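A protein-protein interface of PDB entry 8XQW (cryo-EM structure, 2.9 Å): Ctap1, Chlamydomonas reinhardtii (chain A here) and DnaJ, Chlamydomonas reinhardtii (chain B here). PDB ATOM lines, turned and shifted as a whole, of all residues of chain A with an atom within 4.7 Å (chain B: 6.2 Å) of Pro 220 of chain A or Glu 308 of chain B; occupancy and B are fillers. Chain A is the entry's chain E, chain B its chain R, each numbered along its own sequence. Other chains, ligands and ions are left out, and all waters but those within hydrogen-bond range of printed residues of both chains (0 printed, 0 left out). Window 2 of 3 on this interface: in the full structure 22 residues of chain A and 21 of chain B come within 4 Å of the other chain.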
ATOM      1  N   LYS A 212     -18.453   1.528  -4.805  1.00  0.00           N
ATOM      2  CA  LYS A 212     -18.550   1.335  -6.241  1.00  0.00           C
ATOM      3  C   LYS A 212     -18.999  -0.066  -6.599  1.00  0.00           C
ATOM      4  O   LYS A 212     -19.821  -0.236  -7.502  1.00  0.00           O
ATOM      5  CB  LYS A 212     -17.201   1.634  -6.884  1.00  0.00           C
ATOM      6  CG  LYS A 212     -17.241   1.774  -8.367  1.00  0.00           C
ATOM      7  CD  LYS A 212     -16.217   2.774  -8.829  1.00  0.00           C
ATOM      8  CE  LYS A 212     -14.896   2.562  -8.144  1.00  0.00           C
ATOM      9  NZ  LYS A 212     -13.938   3.615  -8.547  1.00  0.00           N
ATOM     10  N   HIS A 213     -18.491  -1.077  -5.902  1.00  0.00           N
ATOM     11  CA  HIS A 213     -18.779  -2.459  -6.246  1.00  0.00           C
ATOM     12  C   HIS A 213     -19.819  -3.099  -5.345  1.00  0.00           C
ATOM     13  O   HIS A 213     -20.409  -4.110  -5.731  1.00  0.00           O
ATOM     14  CB  HIS A 213     -17.498  -3.294  -6.192  1.00  0.00           C
ATOM     15  CG  HIS A 213     -16.393  -2.754  -7.042  1.00  0.00           C
ATOM     16  ND1 HIS A 213     -15.146  -2.453  -6.540  1.00  0.00           N
ATOM     17  CD2 HIS A 213     -16.350  -2.456  -8.361  1.00  0.00           C
ATOM     18  CE1 HIS A 213     -14.383  -1.992  -7.513  1.00  0.00           C
ATOM     19  NE2 HIS A 213     -15.089  -1.983  -8.628  1.00  0.00           N
ATOM     20  N   GLY A 218     -23.110   3.639  -7.262  1.00  0.00           N
ATOM     21  CA  GLY A 218     -21.705   4.011  -7.318  1.00  0.00           C
ATOM     22  C   GLY A 218     -21.366   4.678  -8.638  1.00  0.00           C
ATOM     23  O   GLY A 218     -21.996   4.422  -9.663  1.00  0.00           O
ATOM     24  N   TRP A 219     -20.362   5.545  -8.608  1.00  0.00           N
ATOM     25  CA  TRP A 219     -19.971   6.309  -9.778  1.00  0.00           C
ATOM     26  C   TRP A 219     -18.504   6.074 -10.105  1.00  0.00           C
ATOM     27  O   TRP A 219     -17.731   5.686  -9.231  1.00  0.00           O
ATOM     28  CB  TRP A 219     -20.215   7.806  -9.555  1.00  0.00           C
ATOM     29  CG  TRP A 219     -19.210   8.463  -8.676  1.00  0.00           C
ATOM     30  CD1 TRP A 219     -17.939   8.833  -9.005  1.00  0.00           C
ATOM     31  CD2 TRP A 219     -19.395   8.851  -7.324  1.00  0.00           C
ATOM     32  NE1 TRP A 219     -17.315   9.411  -7.933  1.00  0.00           N
ATOM     33  CE2 TRP A 219     -18.192   9.437  -6.889  1.00  0.00           C
ATOM     34  CE3 TRP A 219     -20.457   8.762  -6.441  1.00  0.00           C
ATOM     35  CZ2 TRP A 219     -18.030   9.925  -5.620  1.00  0.00           C
ATOM     36  CZ3 TRP A 219     -20.291   9.238  -5.187  1.00  0.00           C
ATOM     37  CH2 TRP A 219     -19.086   9.814  -4.778  1.00  0.00           C
ATOM     38  N   PRO A 220     -18.089   6.298 -11.345  1.00  0.00           N
ATOM     39  CA  PRO A 220     -16.677   6.182 -11.696  1.00  0.00           C
ATOM     40  C   PRO A 220     -15.963   7.524 -11.661  1.00  0.00           C
ATOM     41  O   PRO A 220     -16.576   8.589 -11.649  1.00  0.00           O
ATOM     42  CB  PRO A 220     -16.746   5.662 -13.129  1.00  0.00           C
ATOM     43  CG  PRO A 220     -17.907   6.391 -13.669  1.00  0.00           C
ATOM     44  CD  PRO A 220     -18.907   6.523 -12.545  1.00  0.00           C
ATOM     45  N   GLY A 221     -14.636   7.451 -11.660  1.00  0.00           N
ATOM     46  CA  GLY A 221     -13.835   8.652 -11.773  1.00  0.00           C
ATOM     47  C   GLY A 221     -13.751   9.418 -10.466  1.00  0.00           C
ATOM     48  O   GLY A 221     -13.823   8.845  -9.383  1.00  0.00           O
ATOM     49  N   TYR A 222     -13.601  10.736 -10.578  1.00  0.00           N
ATOM     50  CA  TYR A 222     -13.419  11.609  -9.432  1.00  0.00           C
ATOM     51  C   TYR A 222     -14.509  12.661  -9.376  1.00  0.00           C
ATOM     52  O   TYR A 222     -15.172  12.952 -10.370  1.00  0.00           O
ATOM     53  CB  TYR A 222     -12.066  12.304  -9.483  1.00  0.00           C
ATOM     54  CG  TYR A 222     -10.923  11.352  -9.389  1.00  0.00           C
ATOM     55  CD1 TYR A 222     -10.476  10.907  -8.173  1.00  0.00           C
ATOM     56  CD2 TYR A 222     -10.302  10.887 -10.520  1.00  0.00           C
ATOM     57  CE1 TYR A 222      -9.454  10.038  -8.088  1.00  0.00           C
ATOM     58  CE2 TYR A 222      -9.279  10.019 -10.444  1.00  0.00           C
ATOM     59  CZ  TYR A 222      -8.853   9.597  -9.226  1.00  0.00           C
ATOM     60  OH  TYR A 222      -7.810   8.716  -9.140  1.00  0.00           O
ATOM     61  N   ALA A 239     -15.616  12.222 -14.267  1.00  0.00           N
ATOM     62  CA  ALA A 239     -15.496  10.897 -14.839  1.00  0.00           C
ATOM     63  C   ALA A 239     -14.612  10.999 -16.071  1.00  0.00           C
ATOM     64  O   ALA A 239     -14.028  12.046 -16.349  1.00  0.00           O
ATOM     65  CB  ALA A 239     -16.869  10.342 -15.187  1.00  0.00           C
ATOM     66  N   CYS B  58     -13.278  -4.130 -19.178  1.00  0.00           N
ATOM     67  CA  CYS B  58     -13.112  -2.865 -18.483  1.00  0.00           C
ATOM     68  C   CYS B  58     -12.460  -1.862 -19.415  1.00  0.00           C
ATOM     69  O   CYS B  58     -11.538  -2.202 -20.155  1.00  0.00           O
ATOM     70  CB  CYS B  58     -12.259  -3.055 -17.235  1.00  0.00           C
ATOM     71  SG  CYS B  58     -12.050  -1.604 -16.201  1.00  0.00           S
ATOM     72  N   ARG B  60     -10.873   0.968 -18.574  1.00  0.00           N
ATOM     73  CA  ARG B  60      -9.699   1.669 -18.075  1.00  0.00           C
ATOM     74  C   ARG B  60      -8.432   0.850 -18.269  1.00  0.00           C
ATOM     75  O   ARG B  60      -7.428   1.365 -18.761  1.00  0.00           O
ATOM     76  CB  ARG B  60      -9.875   2.024 -16.607  1.00  0.00           C
ATOM     77  CG  ARG B  60      -8.673   2.737 -16.078  1.00  0.00           C
ATOM     78  CD  ARG B  60      -8.981   3.591 -14.885  1.00  0.00           C
ATOM     79  NE  ARG B  60      -8.142   3.227 -13.750  1.00  0.00           N
ATOM     80  CZ  ARG B  60      -6.859   3.552 -13.632  1.00  0.00           C
ATOM     81  NH1 ARG B  60      -6.263   4.259 -14.582  1.00  0.00           N
ATOM     82  NH2 ARG B  60      -6.174   3.170 -12.561  1.00  0.00           N
ATOM     83  N   CYS B 306      -6.404  -2.580 -10.848  1.00  0.00           N
ATOM     84  CA  CYS B 306      -7.246  -1.517 -11.372  1.00  0.00           C
ATOM     85  C   CYS B 306      -8.312  -1.164 -10.350  1.00  0.00           C
ATOM     86  O   CYS B 306      -8.785  -2.026  -9.610  1.00  0.00           O
ATOM     87  CB  CYS B 306      -7.892  -1.957 -12.677  1.00  0.00           C
ATOM     88  SG  CYS B 306      -8.888  -0.732 -13.488  1.00  0.00           S
ATOM     89  N   ASN B 307      -8.685   0.108 -10.293  1.00  0.00           N
ATOM     90  CA  ASN B 307      -9.654   0.530  -9.294  1.00  0.00           C
ATOM     91  C   ASN B 307     -11.025   0.832  -9.868  1.00  0.00           C
ATOM     92  O   ASN B 307     -11.897   1.285  -9.127  1.00  0.00           O
ATOM     93  CB  ASN B 307      -9.146   1.751  -8.536  1.00  0.00           C
ATOM     94  CG  ASN B 307      -8.467   2.734  -9.433  1.00  0.00           C
ATOM     95  OD1 ASN B 307      -8.005   2.383 -10.514  1.00  0.00           O
ATOM     96  ND2 ASN B 307      -8.408   3.984  -9.001  1.00  0.00           N
ATOM     97  N   GLU B 308     -11.244   0.601 -11.160  1.00  0.00           N
ATOM     98  CA  GLU B 308     -12.604   0.621 -11.676  1.00  0.00           C
ATOM     99  C   GLU B 308     -13.245  -0.749 -11.544  1.00  0.00           C
ATOM    100  O   GLU B 308     -14.226  -0.918 -10.818  1.00  0.00           O
ATOM    101  CB  GLU B 308     -12.600   1.073 -13.125  1.00  0.00           C
ATOM    102  CG  GLU B 308     -11.898   2.387 -13.322  1.00  0.00           C
ATOM    103  CD  GLU B 308     -12.795   3.575 -13.039  1.00  0.00           C
ATOM    104  OE1 GLU B 308     -12.416   4.429 -12.210  1.00  0.00           O
ATOM    105  OE2 GLU B 308     -13.877   3.657 -13.652  1.00  0.00           O
ATOM    106  N   CYS B 309     -12.693  -1.738 -12.223  1.00  0.00           N
ATOM    107  CA  CYS B 309     -12.949  -3.117 -11.871  1.00  0.00           C
ATOM    108  C   CYS B 309     -12.169  -3.419 -10.603  1.00  0.00           C
ATOM    109  O   CYS B 309     -11.284  -2.666 -10.203  1.00  0.00           O
ATOM    110  CB  CYS B 309     -12.547  -4.042 -13.012  1.00  0.00           C
ATOM    111  SG  CYS B 309     -10.895  -3.767 -13.652  1.00  0.00           S
ATOM    112  N   GLY B 310     -12.492  -4.510  -9.942  1.00  0.00           N
ATOM    113  CA  GLY B 310     -11.670  -4.821  -8.796  1.00  0.00           C
ATOM    114  C   GLY B 310     -10.389  -5.515  -9.135  1.00  0.00           C
ATOM    115  O   GLY B 310      -9.647  -5.917  -8.239  1.00  0.00           O
ATOM    116  N   GLY B 311     -10.105  -5.654 -10.418  1.00  0.00           N
ATOM    117  CA  GLY B 311      -9.163  -6.629 -10.916  1.00  0.00           C
ATOM    118  C   GLY B 311      -9.821  -7.727 -11.713  1.00  0.00           C
ATOM    119  O   GLY B 311      -9.123  -8.508 -12.368  1.00  0.00           O
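Of the 8 printed residues of chain A, 4 touch a printed residue of chain B. Of the 8 printed residues of chain B, 4 touch a printed residue of chain A. Printed residues of chain B that touch a printed residue of chain A: Asn 307, Glu 308, Cys 309 and Gly 310.
Among the printed residues, pairs that only touch across the chains: His 213 of chain A with Cys 309 of chain B, His 213 of chain A with Gly 310 of chain B, Pro 220 of chain A with Glu 308 of chain B and Gly 221 of chain A with Glu 308 of chain B.
The guanidinium group (NH2) of Arg 60 of chain B is in hydrogen-bond range of the side-chain amide oxygen (OD1) of Asn 307 of chain B (2.9 Å). The side-chain sulfur of Cys 306 of chain B sits close to the backbone NH of Glu 308 of chain B (3.6 Å).
The backbone carbonyl oxygen (O) of Asn 307 of chain B is in hydrogen-bond range of the side-chain amino group (NZ) of Lys 212 of chain A. The backbone carbonyl oxygen (O) of Glu 308 of chain B lies within hydrogen-bond range of a ring nitrogen (NE2) of His 213 of chain A.
Trp 219 of chain A touches none of the printed residues of chain B. Pro 220 of chain A touches just one residue of chain B: Glu 308. Of the printed residues of chain B, Gly 221 of chain A touches Glu 308 (3.8 Å). Cys 306 of chain B touches none of the printed residues of chain A. Glu 308 of chain B touches just these residues of chain A: His 213 (2.6 Å), Pro 220 (3.5 Å) and Gly 221 (3.8 Å). Printed residues of chain A within 4 Å of Cys 309 of chain B: His 213. The nearest printed residue of chain B that does not touch Pro 220 of chain A is Asn 307 of chain B (7.3 Å).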
